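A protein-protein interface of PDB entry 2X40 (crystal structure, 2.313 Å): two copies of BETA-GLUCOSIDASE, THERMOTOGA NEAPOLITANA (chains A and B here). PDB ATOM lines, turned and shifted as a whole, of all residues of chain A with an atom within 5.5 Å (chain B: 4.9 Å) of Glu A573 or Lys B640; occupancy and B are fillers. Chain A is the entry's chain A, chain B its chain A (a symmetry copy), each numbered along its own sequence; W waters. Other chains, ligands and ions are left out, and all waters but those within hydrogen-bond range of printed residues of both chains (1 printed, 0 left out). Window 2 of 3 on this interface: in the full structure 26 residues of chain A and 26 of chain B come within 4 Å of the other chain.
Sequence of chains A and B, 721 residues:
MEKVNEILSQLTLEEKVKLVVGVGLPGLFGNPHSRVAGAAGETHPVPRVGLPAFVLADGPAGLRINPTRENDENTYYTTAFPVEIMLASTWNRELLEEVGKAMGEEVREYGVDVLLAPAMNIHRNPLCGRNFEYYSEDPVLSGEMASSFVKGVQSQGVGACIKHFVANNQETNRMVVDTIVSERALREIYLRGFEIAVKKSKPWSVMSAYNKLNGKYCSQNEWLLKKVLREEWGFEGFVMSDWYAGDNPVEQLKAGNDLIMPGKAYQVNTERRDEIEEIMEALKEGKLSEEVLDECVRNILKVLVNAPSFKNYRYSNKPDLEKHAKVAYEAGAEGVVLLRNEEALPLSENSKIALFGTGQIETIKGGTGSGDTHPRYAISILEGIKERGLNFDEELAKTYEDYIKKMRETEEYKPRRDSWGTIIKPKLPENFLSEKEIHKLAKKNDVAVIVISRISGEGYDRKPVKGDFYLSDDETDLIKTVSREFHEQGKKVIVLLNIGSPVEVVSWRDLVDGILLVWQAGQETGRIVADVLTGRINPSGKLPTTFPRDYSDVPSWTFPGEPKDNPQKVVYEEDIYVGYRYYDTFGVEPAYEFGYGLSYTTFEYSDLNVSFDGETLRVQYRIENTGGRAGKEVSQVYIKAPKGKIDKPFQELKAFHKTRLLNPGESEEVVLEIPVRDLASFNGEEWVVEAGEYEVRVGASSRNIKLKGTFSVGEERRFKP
O of Thr B585 lies within hydrogen-bond range of NE1 of Trp A557 (2.6 Å).
The side-chain carboxylate of Glu A573 lies within salt-bridge range of the side-chain amino group of Lys B640, at 2.7 Å.
The side-chain amino group (NZ) of Lys B643 lies within salt-bridge range of the side-chain carboxylate (OE1) of Glu A573 (2.9 Å).
NE of Arg A124 lies within salt-bridge range of OE1 of Glu A574, at 2.8 Å.
The side-chain hydroxyl of Thr A558 sits at hydrogen-bond distance from the backbone carbonyl oxygen of Val A571 (2.8 Å).
N of Phe B650 lies within hydrogen-bond range of OG1 of Thr B585 (2.9 Å).
The backbone carbonyl oxygen of Phe B650 lies close to the side-chain amino group of Lys B640 (3.2 Å).
The backbone NH (N) of Lys B640 is in hydrogen-bond range of the backbone carbonyl oxygen (O) of Glu B695, at 2.9 Å.
The side-chain amino group of Lys B648 sits at hydrogen-bond distance from the backbone carbonyl oxygen of Lys B643, at 3.1 Å.
Among the printed residues, pairs that only touch across the chains: Trp A557 with Phe B586 (3.3 Å), Val A571 with Lys B643 (3.7 Å), Glu A573 with Thr B585 (3.2 Å), Glu A573 with Phe B650 (3.5 Å) and Glu A574 with Phe B586 (3.5 Å).
Printed residues of chain B within 4 Å of Trp A557: Thr B585 (2.6 Å) and Phe B586 (3.3 Å).
Printed residues of chain B within 4 Å of Val A571: Lys B643 (3.7 Å).
Printed residues of chain B within 4 Å of Glu A573: Thr B585 (3.2 Å), Lys B640 (2.7 Å), Lys B643 (2.9 Å) and Phe B650 (3.5 Å).
Of the printed residues of chain B, Glu A574 touches Phe B586.
Asp A575 touches none of the printed residues of chain B.
Of the printed residues of chain A, Thr B585 touches Trp A557 and Glu A573.
Of the printed residues of chain A, Lys B643 touches Val A571 (3.7 Å) and Glu A573 (2.9 Å).
Lys B648 touches none of the printed residues of chain A.
The nearest residue of chain B that does not touch Glu A573 is Lys B648 (4.7 Å).
The nearest residue of chain A that does not touch Lys B640 is Val A571 (4.8 Å).
The nearest printed residue of chain B that does not touch Trp A557 is Phe B650 (4.3 Å).
Hydrophobic or aromatic side chains of chain A within 4 Å of the printed part of chain B: Trp A557 and Val A571.
Printed residues of chain B that touch a printed residue of chain A: Thr B585, Phe B586, Lys B640, Lys B643 and Phe B650.
Hydrophobic or aromatic side chains of chain B that line the printed part of chain A: Phe B586 and Phe B650.
No position is printed for both chains.
Of the 8 pairs that touch across the chains among the printed residues, none has its exchanged pair printed and touching as well.
Water W1 lies within hydrogen-bond range of OD2 of Asp A575 (2.8 Å), NZ of Lys B643 (2.9 Å) and N of Lys B648 (3.2 Å).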
ATOM      1  N   ARG A 124     -40.522  -1.242 -36.582  1.00  0.00           N
ATOM      2  CA  ARG A 124     -39.294  -0.716 -35.997  1.00  0.00           C
ATOM      3  C   ARG A 124     -38.546   0.118 -37.033  1.00  0.00           C
ATOM      4  O   ARG A 124     -38.041   1.203 -36.737  1.00  0.00           O
ATOM      5  CB  ARG A 124     -38.402  -1.851 -35.484  1.00  0.00           C
ATOM      6  CG  ARG A 124     -37.033  -1.372 -35.018  1.00  0.00           C
ATOM      7  CD  ARG A 124     -36.111  -2.478 -34.510  1.00  0.00           C
ATOM      8  NE  ARG A 124     -34.867  -1.877 -34.015  1.00  0.00           N
ATOM      9  CZ  ARG A 124     -33.664  -2.055 -34.557  1.00  0.00           C
ATOM     10  NH1 ARG A 124     -33.506  -2.850 -35.604  1.00  0.00           N
ATOM     11  NH2 ARG A 124     -32.611  -1.443 -34.041  1.00  0.00           N
ATOM     12  N   TRP A 557     -31.051   2.268 -36.413  1.00  0.00           N
ATOM     13  CA  TRP A 557     -29.895   2.251 -37.303  1.00  0.00           C
ATOM     14  C   TRP A 557     -29.172   0.902 -37.372  1.00  0.00           C
ATOM     15  O   TRP A 557     -28.432   0.648 -38.322  1.00  0.00           O
ATOM     16  CB  TRP A 557     -28.896   3.351 -36.897  1.00  0.00           C
ATOM     17  CG  TRP A 557     -28.340   3.203 -35.489  1.00  0.00           C
ATOM     18  CD1 TRP A 557     -28.874   3.711 -34.337  1.00  0.00           C
ATOM     19  CD2 TRP A 557     -27.152   2.491 -35.098  1.00  0.00           C
ATOM     20  NE1 TRP A 557     -28.086   3.370 -33.256  1.00  0.00           N
ATOM     21  CE2 TRP A 557     -27.028   2.617 -33.695  1.00  0.00           C
ATOM     22  CE3 TRP A 557     -26.183   1.760 -35.798  1.00  0.00           C
ATOM     23  CZ2 TRP A 557     -25.971   2.042 -32.976  1.00  0.00           C
ATOM     24  CZ3 TRP A 557     -25.125   1.188 -35.080  1.00  0.00           C
ATOM     25  CH2 TRP A 557     -25.029   1.337 -33.685  1.00  0.00           C
ATOM     26  N   THR A 558     -29.362   0.044 -36.373  1.00  0.00           N
ATOM     27  CA  THR A 558     -28.613  -1.216 -36.339  1.00  0.00           C
ATOM     28  C   THR A 558     -29.177  -2.248 -37.311  1.00  0.00           C
ATOM     29  O   THR A 558     -28.512  -3.225 -37.642  1.00  0.00           O
ATOM     30  CB  THR A 558     -28.548  -1.823 -34.927  1.00  0.00           C
ATOM     31  OG1 THR A 558     -29.862  -2.210 -34.508  1.00  0.00           O
ATOM     32  CG2 THR A 558     -27.944  -0.819 -33.932  1.00  0.00           C
ATOM     33  N   VAL A 571     -29.148  -5.572 -32.055  1.00  0.00           N
ATOM     34  CA  VAL A 571     -29.630  -5.030 -30.794  1.00  0.00           C
ATOM     35  C   VAL A 571     -30.399  -3.729 -30.965  1.00  0.00           C
ATOM     36  O   VAL A 571     -30.015  -2.854 -31.741  1.00  0.00           O
ATOM     37  CB  VAL A 571     -28.534  -4.951 -29.686  1.00  0.00           C
ATOM     38  CG1 VAL A 571     -27.230  -5.575 -30.162  1.00  0.00           C
ATOM     39  CG2 VAL A 571     -28.358  -3.525 -29.168  1.00  0.00           C
ATOM     40  N   TYR A 572     -31.507  -3.628 -30.246  1.00  0.00           N
ATOM     41  CA  TYR A 572     -32.372  -2.473 -30.359  1.00  0.00           C
ATOM     42  C   TYR A 572     -31.818  -1.332 -29.527  1.00  0.00           C
ATOM     43  O   TYR A 572     -32.321  -1.036 -28.443  1.00  0.00           O
ATOM     44  CB  TYR A 572     -33.794  -2.838 -29.928  1.00  0.00           C
ATOM     45  CG  TYR A 572     -34.490  -3.775 -30.892  1.00  0.00           C
ATOM     46  CD1 TYR A 572     -33.773  -4.476 -31.854  1.00  0.00           C
ATOM     47  CD2 TYR A 572     -35.866  -3.956 -30.843  1.00  0.00           C
ATOM     48  CE1 TYR A 572     -34.408  -5.329 -32.742  1.00  0.00           C
ATOM     49  CE2 TYR A 572     -36.512  -4.814 -31.725  1.00  0.00           C
ATOM     50  CZ  TYR A 572     -35.779  -5.497 -32.670  1.00  0.00           C
ATOM     51  OH  TYR A 572     -36.424  -6.343 -33.543  1.00  0.00           O
ATOM     52  N   GLU A 573     -30.777  -0.690 -30.043  1.00  0.00           N
ATOM     53  CA  GLU A 573     -30.110   0.385 -29.313  1.00  0.00           C
ATOM     54  C   GLU A 573     -31.068   1.528 -28.980  1.00  0.00           C
ATOM     55  O   GLU A 573     -30.984   2.123 -27.903  1.00  0.00           O
ATOM     56  CB  GLU A 573     -28.905   0.898 -30.097  1.00  0.00           C
ATOM     57  CG  GLU A 573     -27.832  -0.161 -30.371  1.00  0.00           C
ATOM     58  CD  GLU A 573     -26.968  -0.482 -29.148  1.00  0.00           C
ATOM     59  OE1 GLU A 573     -27.169   0.138 -28.081  1.00  0.00           O
ATOM     60  OE2 GLU A 573     -26.085  -1.359 -29.259  1.00  0.00           O
ATOM     61  N   GLU A 574     -31.991   1.820 -29.895  1.00  0.00           N
ATOM     62  CA  GLU A 574     -32.911   2.942 -29.715  1.00  0.00           C
ATOM     63  C   GLU A 574     -33.981   2.610 -28.677  1.00  0.00           C
ATOM     64  O   GLU A 574     -34.634   3.503 -28.136  1.00  0.00           O
ATOM     65  CB  GLU A 574     -33.544   3.373 -31.047  1.00  0.00           C
ATOM     66  CG  GLU A 574     -34.683   2.477 -31.539  1.00  0.00           C
ATOM     67  CD  GLU A 574     -34.216   1.098 -31.982  1.00  0.00           C
ATOM     68  OE1 GLU A 574     -35.078   0.218 -32.175  1.00  0.00           O
ATOM     69  OE2 GLU A 574     -32.991   0.890 -32.143  1.00  0.00           O
ATOM     70  N   ASP A 575     -34.157   1.319 -28.411  1.00  0.00           N
ATOM     71  CA  ASP A 575     -34.977   0.891 -27.290  1.00  0.00           C
ATOM     72  C   ASP A 575     -36.417   1.394 -27.429  1.00  0.00           C
ATOM     73  O   ASP A 575     -37.028   1.240 -28.484  1.00  0.00           O
ATOM     74  CB  ASP A 575     -34.348   1.401 -25.991  1.00  0.00           C
ATOM     75  CG  ASP A 575     -34.747   0.576 -24.785  1.00  0.00           C
ATOM     76  OD1 ASP A 575     -35.837   0.830 -24.227  1.00  0.00           O
ATOM     77  OD2 ASP A 575     -33.962  -0.314 -24.385  1.00  0.00           O
ATOM     78  N   THR B 585     -26.041   6.098 -29.401  1.00  0.00           N
ATOM     79  CA  THR B 585     -27.237   5.290 -29.218  1.00  0.00           C
ATOM     80  C   THR B 585     -28.169   5.360 -30.433  1.00  0.00           C
ATOM     81  O   THR B 585     -28.672   4.333 -30.891  1.00  0.00           O
ATOM     82  CB  THR B 585     -27.992   5.691 -27.945  1.00  0.00           C
ATOM     83  OG1 THR B 585     -27.086   5.696 -26.830  1.00  0.00           O
ATOM     84  CG2 THR B 585     -29.132   4.721 -27.674  1.00  0.00           C
ATOM     85  N   PHE B 586     -28.374   6.560 -30.971  1.00  0.00           N
ATOM     86  CA  PHE B 586     -29.311   6.723 -32.084  1.00  0.00           C
ATOM     87  C   PHE B 586     -28.665   6.896 -33.460  1.00  0.00           C
ATOM     88  O   PHE B 586     -29.339   7.219 -34.430  1.00  0.00           O
ATOM     89  CB  PHE B 586     -30.330   7.826 -31.781  1.00  0.00           C
ATOM     90  CG  PHE B 586     -31.056   7.613 -30.491  1.00  0.00           C
ATOM     91  CD1 PHE B 586     -30.725   8.347 -29.366  1.00  0.00           C
ATOM     92  CD2 PHE B 586     -32.031   6.631 -30.384  1.00  0.00           C
ATOM     93  CE1 PHE B 586     -31.373   8.129 -28.168  1.00  0.00           C
ATOM     94  CE2 PHE B 586     -32.680   6.408 -29.184  1.00  0.00           C
ATOM     95  CZ  PHE B 586     -32.353   7.161 -28.077  1.00  0.00           C
ATOM     96  N   TYR B 638     -14.549   2.809 -22.366  1.00  0.00           N
ATOM     97  CA  TYR B 638     -15.996   2.887 -22.347  1.00  0.00           C
ATOM     98  C   TYR B 638     -16.537   1.511 -22.000  1.00  0.00           C
ATOM     99  O   TYR B 638     -16.002   0.495 -22.443  1.00  0.00           O
ATOM    100  CB  TYR B 638     -16.530   3.323 -23.717  1.00  0.00           C
ATOM    101  CG  TYR B 638     -16.072   4.697 -24.158  1.00  0.00           C
ATOM    102  CD1 TYR B 638     -14.874   4.868 -24.845  1.00  0.00           C
ATOM    103  CD2 TYR B 638     -16.842   5.824 -23.897  1.00  0.00           C
ATOM    104  CE1 TYR B 638     -14.452   6.126 -25.251  1.00  0.00           C
ATOM    105  CE2 TYR B 638     -16.430   7.079 -24.292  1.00  0.00           C
ATOM    106  CZ  TYR B 638     -15.233   7.227 -24.971  1.00  0.00           C
ATOM    107  OH  TYR B 638     -14.826   8.477 -25.371  1.00  0.00           O
ATOM    108  N   ILE B 639     -17.588   1.475 -21.194  1.00  0.00           N
ATOM    109  CA  ILE B 639     -18.269   0.221 -20.930  1.00  0.00           C
ATOM    110  C   ILE B 639     -19.618   0.195 -21.643  1.00  0.00           C
ATOM    111  O   ILE B 639     -20.411   1.131 -21.542  1.00  0.00           O
ATOM    112  CB  ILE B 639     -18.478  -0.008 -19.432  1.00  0.00           C
ATOM    113  CG1 ILE B 639     -17.149   0.141 -18.693  1.00  0.00           C
ATOM    114  CG2 ILE B 639     -19.081  -1.382 -19.189  1.00  0.00           C
ATOM    115  CD1 ILE B 639     -16.077  -0.782 -19.209  1.00  0.00           C
ATOM    116  N   LYS B 640     -19.860  -0.875 -22.386  1.00  0.00           N
ATOM    117  CA  LYS B 640     -21.161  -1.098 -22.990  1.00  0.00           C
ATOM    118  C   LYS B 640     -21.880  -2.134 -22.134  1.00  0.00           C
ATOM    119  O   LYS B 640     -21.516  -3.307 -22.134  1.00  0.00           O
ATOM    120  CB  LYS B 640     -20.996  -1.586 -24.432  1.00  0.00           C
ATOM    121  CG  LYS B 640     -22.300  -1.844 -25.172  1.00  0.00           C
ATOM    122  CD  LYS B 640     -22.124  -1.729 -26.691  1.00  0.00           C
ATOM    123  CE  LYS B 640     -23.398  -2.144 -27.431  1.00  0.00           C
ATOM    124  NZ  LYS B 640     -24.613  -1.414 -26.961  1.00  0.00           N
ATOM    125  N   ALA B 641     -22.868  -1.688 -21.366  1.00  0.00           N
ATOM    126  CA  ALA B 641     -23.611  -2.594 -20.501  1.00  0.00           C
ATOM    127  C   ALA B 641     -24.642  -3.359 -21.327  1.00  0.00           C
ATOM    128  O   ALA B 641     -25.076  -2.877 -22.374  1.00  0.00           O
ATOM    129  CB  ALA B 641     -24.283  -1.827 -19.380  1.00  0.00           C
ATOM    130  N   PRO B 642     -25.024  -4.561 -20.867  1.00  0.00           N
ATOM    131  CA  PRO B 642     -26.029  -5.359 -21.580  1.00  0.00           C
ATOM    132  C   PRO B 642     -27.391  -4.662 -21.571  1.00  0.00           C
ATOM    133  O   PRO B 642     -27.641  -3.829 -20.696  1.00  0.00           O
ATOM    134  CB  PRO B 642     -26.091  -6.650 -20.765  1.00  0.00           C
ATOM    135  CG  PRO B 642     -25.620  -6.261 -19.392  1.00  0.00           C
ATOM    136  CD  PRO B 642     -24.576  -5.211 -19.622  1.00  0.00           C
ATOM    137  N   LYS B 643     -28.261  -4.991 -22.522  1.00  0.00           N
ATOM    138  CA  LYS B 643     -29.580  -4.361 -22.550  1.00  0.00           C
ATOM    139  C   LYS B 643     -30.404  -4.698 -21.298  1.00  0.00           C
ATOM    140  O   LYS B 643     -30.992  -3.813 -20.677  1.00  0.00           O
ATOM    141  CB  LYS B 643     -30.332  -4.677 -23.852  1.00  0.00           C
ATOM    142  CG  LYS B 643     -29.728  -3.987 -25.070  1.00  0.00           C
ATOM    143  CD  LYS B 643     -29.435  -2.525 -24.745  1.00  0.00           C
ATOM    144  CE  LYS B 643     -28.783  -1.782 -25.897  1.00  0.00           C
ATOM    145  NZ  LYS B 643     -28.582  -0.341 -25.566  1.00  0.00           N
ATOM    146  N   LYS B 648     -30.408   1.775 -21.855  1.00  0.00           N
ATOM    147  CA  LYS B 648     -29.128   2.378 -21.500  1.00  0.00           C
ATOM    148  C   LYS B 648     -28.458   2.945 -22.737  1.00  0.00           C
ATOM    149  O   LYS B 648     -28.695   2.470 -23.850  1.00  0.00           O
ATOM    150  CB  LYS B 648     -28.196   1.341 -20.869  1.00  0.00           C
ATOM    151  CG  LYS B 648     -28.750   0.628 -19.645  1.00  0.00           C
ATOM    152  CD  LYS B 648     -27.714  -0.348 -19.097  1.00  0.00           C
ATOM    153  CE  LYS B 648     -28.296  -1.277 -18.039  1.00  0.00           C
ATOM    154  NZ  LYS B 648     -29.279  -2.226 -18.635  1.00  0.00           N
ATOM    155  N   PHE B 650     -25.659   3.544 -25.606  1.00  0.00           N
ATOM    156  CA  PHE B 650     -24.841   2.586 -26.333  1.00  0.00           C
ATOM    157  C   PHE B 650     -23.607   2.195 -25.510  1.00  0.00           C
ATOM    158  O   PHE B 650     -23.315   1.012 -25.337  1.00  0.00           O
ATOM    159  CB  PHE B 650     -24.459   3.174 -27.701  1.00  0.00           C
ATOM    160  CG  PHE B 650     -23.459   2.355 -28.465  1.00  0.00           C
ATOM    161  CD1 PHE B 650     -23.875   1.323 -29.294  1.00  0.00           C
ATOM    162  CD2 PHE B 650     -22.101   2.630 -28.369  1.00  0.00           C
ATOM    163  CE1 PHE B 650     -22.954   0.567 -30.004  1.00  0.00           C
ATOM    164  CE2 PHE B 650     -21.180   1.888 -29.076  1.00  0.00           C
ATOM    165  CZ  PHE B 650     -21.604   0.852 -29.896  1.00  0.00           C
ATOM    166  N   GLN B 651     -22.897   3.194 -24.993  1.00  0.00           N
ATOM    167  CA  GLN B 651     -21.753   2.952 -24.112  1.00  0.00           C
ATOM    168  C   GLN B 651     -21.563   4.145 -23.179  1.00  0.00           C
ATOM    169  O   GLN B 651     -22.137   5.207 -23.402  1.00  0.00           O
ATOM    170  CB  GLN B 651     -20.478   2.756 -24.935  1.00  0.00           C
ATOM    171  CG  GLN B 651     -20.005   4.046 -25.562  1.00  0.00           C
ATOM    172  CD  GLN B 651     -18.955   3.859 -26.632  1.00  0.00           C
ATOM    173  OE1 GLN B 651     -18.284   2.823 -26.713  1.00  0.00           O
ATOM    174  NE2 GLN B 651     -18.799   4.880 -27.466  1.00  0.00           N
ATOM    175  N   GLU B 693     -23.384  -9.984 -19.441  1.00  0.00           N
ATOM    176  CA  GLU B 693     -22.112  -9.728 -20.091  1.00  0.00           C
ATOM    177  C   GLU B 693     -21.924  -8.243 -20.422  1.00  0.00           C
ATOM    178  O   GLU B 693     -22.805  -7.610 -21.005  1.00  0.00           O
ATOM    179  CB  GLU B 693     -21.996 -10.586 -21.351  1.00  0.00           C
ATOM    180  CG  GLU B 693     -20.597 -10.642 -21.934  1.00  0.00           C
ATOM    181  CD  GLU B 693     -20.462 -11.686 -23.025  1.00  0.00           C
ATOM    182  OE1 GLU B 693     -21.024 -11.477 -24.124  1.00  0.00           O
ATOM    183  OE2 GLU B 693     -19.788 -12.712 -22.782  1.00  0.00           O
ATOM    184  N   TYR B 694     -20.767  -7.705 -20.037  1.00  0.00           N
ATOM    185  CA  TYR B 694     -20.398  -6.311 -20.286  1.00  0.00           C
ATOM    186  C   TYR B 694     -19.234  -6.230 -21.260  1.00  0.00           C
ATOM    187  O   TYR B 694     -18.335  -7.065 -21.219  1.00  0.00           O
ATOM    188  CB  TYR B 694     -19.954  -5.657 -18.982  1.00  0.00           C
ATOM    189  CG  TYR B 694     -21.077  -5.316 -18.039  1.00  0.00           C
ATOM    190  CD1 TYR B 694     -21.762  -6.311 -17.350  1.00  0.00           C
ATOM    191  CD2 TYR B 694     -21.445  -3.993 -17.828  1.00  0.00           C
ATOM    192  CE1 TYR B 694     -22.791  -5.992 -16.480  1.00  0.00           C
ATOM    193  CE2 TYR B 694     -22.470  -3.664 -16.968  1.00  0.00           C
ATOM    194  CZ  TYR B 694     -23.139  -4.664 -16.294  1.00  0.00           C
ATOM    195  OH  TYR B 694     -24.157  -4.326 -15.438  1.00  0.00           O
ATOM    196  N   GLU B 695     -19.229  -5.215 -22.117  1.00  0.00           N
ATOM    197  CA  GLU B 695     -18.104  -5.023 -23.026  1.00  0.00           C
ATOM    198  C   GLU B 695     -17.193  -3.886 -22.571  1.00  0.00           C
ATOM    199  O   GLU B 695     -17.656  -2.804 -22.205  1.00  0.00           O
ATOM    200  CB  GLU B 695     -18.566  -4.774 -24.466  1.00  0.00           C
ATOM    201  CG  GLU B 695     -17.405  -4.549 -25.448  1.00  0.00           C
ATOM    202  CD  GLU B 695     -17.847  -4.444 -26.908  1.00  0.00           C
ATOM    203  OE1 GLU B 695     -17.308  -5.206 -27.740  1.00  0.00           O
ATOM    204  OE2 GLU B 695     -18.720  -3.603 -27.231  1.00  0.00           O
ATOM    205  N   ARG B 697     -14.517  -1.315 -23.904  1.00  0.00           N
ATOM    206  CA  ARG B 697     -14.115  -0.706 -25.159  1.00  0.00           C
ATOM    207  C   ARG B 697     -13.045   0.355 -24.891  1.00  0.00           C
ATOM    208  O   ARG B 697     -13.351   1.460 -24.448  1.00  0.00           O
ATOM    209  CB  ARG B 697     -15.337  -0.106 -25.869  1.00  0.00           C
ATOM    210  CG  ARG B 697     -16.415  -1.133 -26.183  1.00  0.00           C
ATOM    211  CD  ARG B 697     -17.781  -0.501 -26.469  1.00  0.00           C
ATOM    212  NE  ARG B 697     -17.799   0.274 -27.705  1.00  0.00           N
ATOM    213  CZ  ARG B 697     -17.825  -0.259 -28.923  1.00  0.00           C
ATOM    214  NH1 ARG B 697     -17.829  -1.579 -29.076  1.00  0.00           N
ATOM    215  NH2 ARG B 697     -17.835   0.530 -29.991  1.00  0.00           N
HETATM  216  O   HOH W   1     -31.229   0.179 -24.499  1.00  0.00           O
